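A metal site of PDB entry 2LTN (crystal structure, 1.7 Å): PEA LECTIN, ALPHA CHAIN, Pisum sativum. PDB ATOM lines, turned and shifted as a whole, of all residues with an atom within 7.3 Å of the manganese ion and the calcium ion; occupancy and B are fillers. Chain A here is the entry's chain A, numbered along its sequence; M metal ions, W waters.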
ATOM      1  N   ASP A  81      -4.255   1.385  11.390  1.00  0.00           N
ATOM      2  CA  ASP A  81      -2.993   1.088  10.900  1.00  0.00           C
ATOM      3  C   ASP A  81      -1.921   0.525  11.813  1.00  0.00           C
ATOM      4  O   ASP A  81      -1.137  -0.435  11.560  1.00  0.00           O
ATOM      5  CB  ASP A  81      -2.362   1.855   9.729  1.00  0.00           C
ATOM      6  CG  ASP A  81      -2.963   1.477   8.399  1.00  0.00           C
ATOM      7  OD1 ASP A  81      -3.841   2.138   7.839  1.00  0.00           O
ATOM      8  OD2 ASP A  81      -2.495   0.450   7.773  1.00  0.00           O
ATOM      9  N   GLY A  82      -1.749   1.255  12.941  1.00  0.00           N
ATOM     10  CA  GLY A  82      -0.769   0.830  13.972  1.00  0.00           C
ATOM     11  C   GLY A  82      -0.185   2.157  14.634  1.00  0.00           C
ATOM     12  O   GLY A  82      -0.794   3.171  14.386  1.00  0.00           O
ATOM     13  N   GLY A  98      -1.617   6.165   6.834  1.00  0.00           N
ATOM     14  CA  GLY A  98      -2.063   4.731   6.551  1.00  0.00           C
ATOM     15  C   GLY A  98      -0.972   3.771   6.960  1.00  0.00           C
ATOM     16  O   GLY A  98      -0.495   3.826   8.055  1.00  0.00           O
ATOM     17  N   GLY A  99      -0.662   2.815   5.962  1.00  0.00           N
ATOM     18  CA  GLY A  99       0.345   1.822   6.298  1.00  0.00           C
ATOM     19  C   GLY A  99       1.756   2.247   6.619  1.00  0.00           C
ATOM     20  O   GLY A  99       2.581   1.504   7.117  1.00  0.00           O
ATOM     21  N   TYR A 100       2.031   3.560   6.289  1.00  0.00           N
ATOM     22  CA  TYR A 100       3.334   4.174   6.524  1.00  0.00           C
ATOM     23  C   TYR A 100       3.488   4.780   7.949  1.00  0.00           C
ATOM     24  O   TYR A 100       4.603   5.158   8.317  1.00  0.00           O
ATOM     25  CB  TYR A 100       3.649   5.212   5.446  1.00  0.00           C
ATOM     26  CG  TYR A 100       3.788   4.554   4.053  1.00  0.00           C
ATOM     27  CD1 TYR A 100       4.980   3.994   3.676  1.00  0.00           C
ATOM     28  CD2 TYR A 100       2.669   4.499   3.245  1.00  0.00           C
ATOM     29  CE1 TYR A 100       5.095   3.437   2.381  1.00  0.00           C
ATOM     30  CE2 TYR A 100       2.747   3.863   1.985  1.00  0.00           C
ATOM     31  CZ  TYR A 100       3.996   3.392   1.575  1.00  0.00           C
ATOM     32  OH  TYR A 100       4.074   2.822   0.311  1.00  0.00           O
ATOM     33  N   LEU A 101       2.407   4.697   8.669  1.00  0.00           N
ATOM     34  CA  LEU A 101       2.354   5.000  10.103  1.00  0.00           C
ATOM     35  C   LEU A 101       2.715   6.464  10.447  1.00  0.00           C
ATOM     36  O   LEU A 101       3.077   6.686  11.643  1.00  0.00           O
ATOM     37  CB  LEU A 101       3.195   3.958  10.930  1.00  0.00           C
ATOM     38  CG  LEU A 101       2.720   2.457  10.654  1.00  0.00           C
ATOM     39  CD1 LEU A 101       3.616   1.510  11.430  1.00  0.00           C
ATOM     40  CD2 LEU A 101       1.269   2.357  10.960  1.00  0.00           C
ATOM     41  N   GLU A 119       7.526  -0.252  15.595  1.00  0.00           N
ATOM     42  CA  GLU A 119       6.145  -0.283  15.185  1.00  0.00           C
ATOM     43  C   GLU A 119       5.317  -1.360  15.808  1.00  0.00           C
ATOM     44  O   GLU A 119       5.882  -2.383  16.132  1.00  0.00           O
ATOM     45  CB  GLU A 119       5.996  -0.311  13.643  1.00  0.00           C
ATOM     46  CG  GLU A 119       6.628  -1.715  13.162  1.00  0.00           C
ATOM     47  CD  GLU A 119       6.278  -1.900  11.720  1.00  0.00           C
ATOM     48  OE1 GLU A 119       5.702  -2.973  11.359  1.00  0.00           O
ATOM     49  OE2 GLU A 119       6.501  -1.016  10.888  1.00  0.00           O
ATOM     50  N   PHE A 120       4.090  -1.128  16.061  1.00  0.00           N
ATOM     51  CA  PHE A 120       3.054  -2.058  16.598  1.00  0.00           C
ATOM     52  C   PHE A 120       2.022  -1.966  15.486  1.00  0.00           C
ATOM     53  O   PHE A 120       1.163  -1.099  15.369  1.00  0.00           O
ATOM     54  CB  PHE A 120       2.527  -1.643  17.994  1.00  0.00           C
ATOM     55  CG  PHE A 120       3.637  -1.487  18.976  1.00  0.00           C
ATOM     56  CD1 PHE A 120       4.396  -0.275  18.969  1.00  0.00           C
ATOM     57  CD2 PHE A 120       4.029  -2.506  19.846  1.00  0.00           C
ATOM     58  CE1 PHE A 120       5.436  -0.097  19.823  1.00  0.00           C
ATOM     59  CE2 PHE A 120       5.103  -2.335  20.739  1.00  0.00           C
ATOM     60  CZ  PHE A 120       5.800  -1.111  20.709  1.00  0.00           C
ATOM     61  N   ASP A 121       2.227  -2.942  14.542  1.00  0.00           N
ATOM     62  CA  ASP A 121       1.513  -2.894  13.236  1.00  0.00           C
ATOM     63  C   ASP A 121       0.287  -3.802  13.209  1.00  0.00           C
ATOM     64  O   ASP A 121       0.460  -4.986  13.495  1.00  0.00           O
ATOM     65  CB  ASP A 121       2.605  -3.246  12.182  1.00  0.00           C
ATOM     66  CG  ASP A 121       2.094  -3.117  10.775  1.00  0.00           C
ATOM     67  OD1 ASP A 121       0.843  -2.945  10.549  1.00  0.00           O
ATOM     68  OD2 ASP A 121       2.954  -3.111   9.888  1.00  0.00           O
ATOM     69  N   THR A 122      -0.855  -3.227  13.024  1.00  0.00           N
ATOM     70  CA  THR A 122      -2.118  -3.987  13.192  1.00  0.00           C
ATOM     71  C   THR A 122      -2.719  -4.410  11.866  1.00  0.00           C
ATOM     72  O   THR A 122      -3.808  -5.016  11.966  1.00  0.00           O
ATOM     73  CB  THR A 122      -3.115  -3.155  14.102  1.00  0.00           C
ATOM     74  OG1 THR A 122      -3.322  -1.897  13.351  1.00  0.00           O
ATOM     75  CG2 THR A 122      -2.656  -2.979  15.532  1.00  0.00           C
ATOM     76  N   PHE A 123      -2.106  -3.999  10.797  1.00  0.00           N
ATOM     77  CA  PHE A 123      -2.778  -4.302   9.472  1.00  0.00           C
ATOM     78  C   PHE A 123      -1.727  -4.781   8.520  1.00  0.00           C
ATOM     79  O   PHE A 123      -0.674  -4.210   8.321  1.00  0.00           O
ATOM     80  CB  PHE A 123      -3.557  -3.083   8.974  1.00  0.00           C
ATOM     81  CG  PHE A 123      -4.105  -3.137   7.591  1.00  0.00           C
ATOM     82  CD1 PHE A 123      -3.447  -2.765   6.459  1.00  0.00           C
ATOM     83  CD2 PHE A 123      -5.480  -3.585   7.507  1.00  0.00           C
ATOM     84  CE1 PHE A 123      -4.036  -2.797   5.208  1.00  0.00           C
ATOM     85  CE2 PHE A 123      -6.101  -3.624   6.223  1.00  0.00           C
ATOM     86  CZ  PHE A 123      -5.330  -3.298   5.117  1.00  0.00           C
ATOM     87  N   TYR A 124      -2.108  -5.922   7.790  1.00  0.00           N
ATOM     88  CA  TYR A 124      -1.107  -6.475   6.833  1.00  0.00           C
ATOM     89  C   TYR A 124      -1.136  -5.776   5.519  1.00  0.00           C
ATOM     90  O   TYR A 124      -2.178  -5.705   4.822  1.00  0.00           O
ATOM     91  CB  TYR A 124      -1.576  -7.988   6.638  1.00  0.00           C
ATOM     92  CG  TYR A 124      -0.871  -8.624   5.451  1.00  0.00           C
ATOM     93  CD1 TYR A 124       0.480  -8.904   5.516  1.00  0.00           C
ATOM     94  CD2 TYR A 124      -1.598  -8.967   4.330  1.00  0.00           C
ATOM     95  CE1 TYR A 124       1.152  -9.487   4.440  1.00  0.00           C
ATOM     96  CE2 TYR A 124      -0.948  -9.593   3.228  1.00  0.00           C
ATOM     97  CZ  TYR A 124       0.395  -9.862   3.319  1.00  0.00           C
ATOM     98  OH  TYR A 124       1.026 -10.452   2.233  1.00  0.00           O
ATOM     99  N   ASN A 125       0.008  -5.207   5.193  1.00  0.00           N
ATOM    100  CA  ASN A 125       0.251  -4.516   3.910  1.00  0.00           C
ATOM    101  C   ASN A 125       1.086  -5.551   3.079  1.00  0.00           C
ATOM    102  O   ASN A 125       2.232  -5.751   3.377  1.00  0.00           O
ATOM    103  CB  ASN A 125       1.062  -3.196   4.085  1.00  0.00           C
ATOM    104  CG  ASN A 125       0.194  -2.192   4.862  1.00  0.00           C
ATOM    105  OD1 ASN A 125       0.240  -2.107   6.089  1.00  0.00           O
ATOM    106  ND2 ASN A 125      -0.657  -1.498   4.118  1.00  0.00           N
ATOM    107  N   ALA A 126       0.339  -6.097   2.081  1.00  0.00           N
ATOM    108  CA  ALA A 126       1.073  -7.129   1.248  1.00  0.00           C
ATOM    109  C   ALA A 126       2.361  -6.725   0.659  1.00  0.00           C
ATOM    110  O   ALA A 126       3.323  -7.607   0.523  1.00  0.00           O
ATOM    111  CB  ALA A 126       0.059  -7.578   0.159  1.00  0.00           C
ATOM    112  N   TRP A 128       4.943  -5.217   1.812  1.00  0.00           N
ATOM    113  CA  TRP A 128       6.069  -5.305   2.701  1.00  0.00           C
ATOM    114  C   TRP A 128       5.900  -5.946   4.043  1.00  0.00           C
ATOM    115  O   TRP A 128       7.033  -6.192   4.583  1.00  0.00           O
ATOM    116  CB  TRP A 128       6.638  -3.800   2.885  1.00  0.00           C
ATOM    117  CG  TRP A 128       5.609  -2.962   3.626  1.00  0.00           C
ATOM    118  CD1 TRP A 128       5.342  -2.950   4.965  1.00  0.00           C
ATOM    119  CD2 TRP A 128       4.816  -1.915   3.047  1.00  0.00           C
ATOM    120  NE1 TRP A 128       4.318  -2.102   5.211  1.00  0.00           N
ATOM    121  CE2 TRP A 128       3.992  -1.425   4.095  1.00  0.00           C
ATOM    122  CE3 TRP A 128       4.680  -1.428   1.751  1.00  0.00           C
ATOM    123  CZ2 TRP A 128       3.056  -0.395   3.900  1.00  0.00           C
ATOM    124  CZ3 TRP A 128       3.763  -0.410   1.560  1.00  0.00           C
ATOM    125  CH2 TRP A 128       2.930   0.080   2.608  1.00  0.00           C
ATOM    126  N   ASP A 129       4.739  -6.221   4.601  1.00  0.00           N
ATOM    127  CA  ASP A 129       4.649  -6.830   5.940  1.00  0.00           C
ATOM    128  C   ASP A 129       4.928  -8.366   5.843  1.00  0.00           C
ATOM    129  O   ASP A 129       4.752  -8.860   4.694  1.00  0.00           O
ATOM    130  CB  ASP A 129       3.264  -6.555   6.538  1.00  0.00           C
ATOM    131  CG  ASP A 129       3.173  -5.083   7.170  1.00  0.00           C
ATOM    132  OD1 ASP A 129       4.292  -4.714   7.588  1.00  0.00           O
ATOM    133  OD2 ASP A 129       2.046  -4.660   7.170  1.00  0.00           O
ATOM    134  N   PRO A 130       5.152  -8.969   6.943  1.00  0.00           N
ATOM    135  CA  PRO A 130       5.392 -10.440   7.006  1.00  0.00           C
ATOM    136  C   PRO A 130       4.209 -11.177   6.331  1.00  0.00           C
ATOM    137  O   PRO A 130       3.045 -10.954   6.630  1.00  0.00           O
ATOM    138  CB  PRO A 130       5.519 -10.718   8.477  1.00  0.00           C
ATOM    139  CG  PRO A 130       6.099  -9.422   9.084  1.00  0.00           C
ATOM    140  CD  PRO A 130       5.380  -8.317   8.284  1.00  0.00           C
ATOM    141  N   ASP A 134       0.279 -11.884  10.218  1.00  0.00           N
ATOM    142  CA  ASP A 134       0.077 -11.650  11.644  1.00  0.00           C
ATOM    143  C   ASP A 134       0.335 -10.113  11.973  1.00  0.00           C
ATOM    144  O   ASP A 134       1.204  -9.590  11.301  1.00  0.00           O
ATOM    145  CB  ASP A 134       1.060 -12.362  12.556  1.00  0.00           C
ATOM    146  CG  ASP A 134       0.808 -13.888  12.590  1.00  0.00           C
ATOM    147  OD1 ASP A 134      -0.302 -14.267  12.145  1.00  0.00           O
ATOM    148  OD2 ASP A 134       1.782 -14.507  13.095  1.00  0.00           O
ATOM    149  N   HIS A 136       2.162  -7.483  14.238  1.00  0.00           N
ATOM    150  CA  HIS A 136       3.525  -7.676  14.642  1.00  0.00           C
ATOM    151  C   HIS A 136       4.196  -6.388  15.238  1.00  0.00           C
ATOM    152  O   HIS A 136       3.612  -5.329  14.931  1.00  0.00           O
ATOM    153  CB  HIS A 136       4.381  -8.070  13.360  1.00  0.00           C
ATOM    154  CG  HIS A 136       4.137  -7.215  12.149  1.00  0.00           C
ATOM    155  ND1 HIS A 136       3.067  -7.396  11.306  1.00  0.00           N
ATOM    156  CD2 HIS A 136       4.862  -6.177  11.627  1.00  0.00           C
ATOM    157  CE1 HIS A 136       3.110  -6.453  10.339  1.00  0.00           C
ATOM    158  NE2 HIS A 136       4.188  -5.748  10.520  1.00  0.00           N
ATOM    159  N   ILE A 137       5.220  -6.684  15.929  1.00  0.00           N
ATOM    160  CA  ILE A 137       6.085  -5.561  16.419  1.00  0.00           C
ATOM    161  C   ILE A 137       7.218  -5.572  15.429  1.00  0.00           C
ATOM    162  O   ILE A 137       7.715  -6.706  15.060  1.00  0.00           O
ATOM    163  CB  ILE A 137       6.591  -5.908  17.855  1.00  0.00           C
ATOM    164  CG1 ILE A 137       5.344  -5.920  18.801  1.00  0.00           C
ATOM    165  CG2 ILE A 137       7.694  -4.911  18.298  1.00  0.00           C
ATOM    166  CD1 ILE A 137       5.661  -6.844  20.043  1.00  0.00           C
ATOM    167  N   GLY A 138       7.811  -4.447  15.040  1.00  0.00           N
ATOM    168  CA  GLY A 138       8.871  -4.302  14.174  1.00  0.00           C
ATOM    169  C   GLY A 138       9.863  -3.145  14.474  1.00  0.00           C
ATOM    170  O   GLY A 138       9.376  -2.191  15.093  1.00  0.00           O
ATOM    171  N   ASP A 140      12.030  -0.539  12.587  1.00  0.00           N
ATOM    172  CA  ASP A 140      12.074   0.119  11.315  1.00  0.00           C
ATOM    173  C   ASP A 140      13.243   1.115  11.264  1.00  0.00           C
ATOM    174  O   ASP A 140      13.349   1.964  12.186  1.00  0.00           O
ATOM    175  CB  ASP A 140      10.788   0.874  10.966  1.00  0.00           C
ATOM    176  CG  ASP A 140       9.551   0.064  10.938  1.00  0.00           C
ATOM    177  OD1 ASP A 140       9.727  -1.200  10.973  1.00  0.00           O
ATOM    178  OD2 ASP A 140       8.396   0.529  10.968  1.00  0.00           O
ATOM    179  N   ILE A 144       9.591   1.492   5.861  1.00  0.00           N
ATOM    180  CA  ILE A 144       8.441   0.829   6.518  1.00  0.00           C
ATOM    181  C   ILE A 144       8.568  -0.750   6.533  1.00  0.00           C
ATOM    182  O   ILE A 144       7.799  -1.421   7.191  1.00  0.00           O
ATOM    183  CB  ILE A 144       7.118   1.259   5.883  1.00  0.00           C
ATOM    184  CG1 ILE A 144       5.907   1.007   6.727  1.00  0.00           C
ATOM    185  CG2 ILE A 144       6.930   0.738   4.409  1.00  0.00           C
ATOM    186  CD1 ILE A 144       5.918   1.713   8.128  1.00  0.00           C
ATOM    187  N   LYS A 145       9.541  -1.165   5.766  1.00  0.00           N
ATOM    188  CA  LYS A 145       9.852  -2.626   5.698  1.00  0.00           C
ATOM    189  C   LYS A 145      10.817  -2.933   6.834  1.00  0.00           C
ATOM    190  O   LYS A 145      12.015  -2.563   6.671  1.00  0.00           O
ATOM    191  CB  LYS A 145      10.451  -3.043   4.328  1.00  0.00           C
ATOM    192  CG  LYS A 145      10.554  -4.631   4.418  1.00  0.00           C
ATOM    193  CD  LYS A 145      10.937  -5.206   3.074  1.00  0.00           C
ATOM    194  CE  LYS A 145      12.389  -5.255   2.761  1.00  0.00           C
ATOM    195  NZ  LYS A 145      13.195  -6.093   3.698  1.00  0.00           N
ATOM    196  N   SER A 146      10.297  -3.481   7.915  1.00  0.00           N
ATOM    197  CA  SER A 146      11.096  -3.714   9.116  1.00  0.00           C
ATOM    198  C   SER A 146      12.356  -4.517   8.958  1.00  0.00           C
ATOM    199  O   SER A 146      12.365  -5.496   8.082  1.00  0.00           O
ATOM    200  CB  SER A 146      10.237  -4.387  10.202  1.00  0.00           C
ATOM    201  OG  SER A 146       9.018  -3.682  10.359  1.00  0.00           O
ATOM    202  N   THR A 149      10.970  -8.459  12.901  1.00  0.00           N
ATOM    203  CA  THR A 149       9.566  -8.438  13.330  1.00  0.00           C
ATOM    204  C   THR A 149       9.332  -9.629  14.252  1.00  0.00           C
ATOM    205  O   THR A 149      10.091 -10.629  14.201  1.00  0.00           O
ATOM    206  CB  THR A 149       8.531  -8.439  12.158  1.00  0.00           C
ATOM    207  OG1 THR A 149       8.842  -9.711  11.398  1.00  0.00           O
ATOM    208  CG2 THR A 149       8.594  -7.251  11.226  1.00  0.00           C
HETATM  209 MN    MN M   1       4.850  -3.861   9.521  1.00  0.00          MN
HETATM  210 CA    CA M   2       1.028  -2.675   8.096  1.00  0.00          CA
HETATM  211  O   HOH W   1      -0.333  -0.849   8.818  1.00  0.00           O
HETATM  212  O   HOH W   2       5.456  -1.903   8.587  1.00  0.00           O
HETATM  213  O   HOH W   3       2.752  -1.128   7.733  1.00  0.00           O
HETATM  214  O   HOH W   4       6.827  -4.600   9.151  1.00  0.00           O
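The side-chain carboxylate (OD2) of Asp 121 is bound to the manganese ion, at 2.1 Å. The manganese ion is bound by water W4 (2.1 Å). The manganese ion is bound by OD1 of Asp 129, at 2.2 Å. The manganese ion is bound by OE1 of Glu 119, 2.2 Å away. A ring nitrogen (NE2) of His 136 binds the manganese ion, 2.2 Å away. Water W2 binds the manganese ion (2.3 Å). The manganese ion has six donor atoms within binding distance.
Four residues have an atom within 4 Å of the manganese ion: Glu 119, Asp 121, Asp 129 and His 136. The nearest printed residue that does not touch the manganese ion is Ser 146 (4.3 Å).
Within 4 Å of the calcium ion: Asp 121, Phe 123, Asn 125 and Asp 129. The nearest printed residue that does not touch the calcium ion is Trp 128 (4.4 Å).
Water W2 lies within hydrogen-bond range of OE2 of Glu 119 and O of Ile 144. Water W3 lies within hydrogen-bond range of the backbone carbonyl oxygen (O) of Gly 99 (2.7 Å) and the indole nitrogen (NE1) of Trp 128 (3.1 Å).
The calcium ion is bound by the side-chain amide oxygen (OD1) of Asn 125 (2.2 Å), the backbone carbonyl oxygen (O) of Phe 123 (2.3 Å), water W3 (2.3 Å), water W1 (2.4 Å), the side-chain carboxylate (OD2) of Asp 129 (2.4 Å), the side-chain carboxylate (OD1) of Asp 121 (2.5 Å) and the side-chain carboxylate (OD2) of Asp 121 (2.7 Å).
A ring nitrogen (ND1) of His 136 is in hydrogen-bond range of the backbone carbonyl oxygen (O) of Asp 134 (2.9 Å). The side-chain carboxylate (OE2) of Glu 119 sits close to the side-chain carboxylate (OD2) of Asp 140. N of Glu 119 lies within hydrogen-bond range of O of Gly 138 (2.7 Å).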
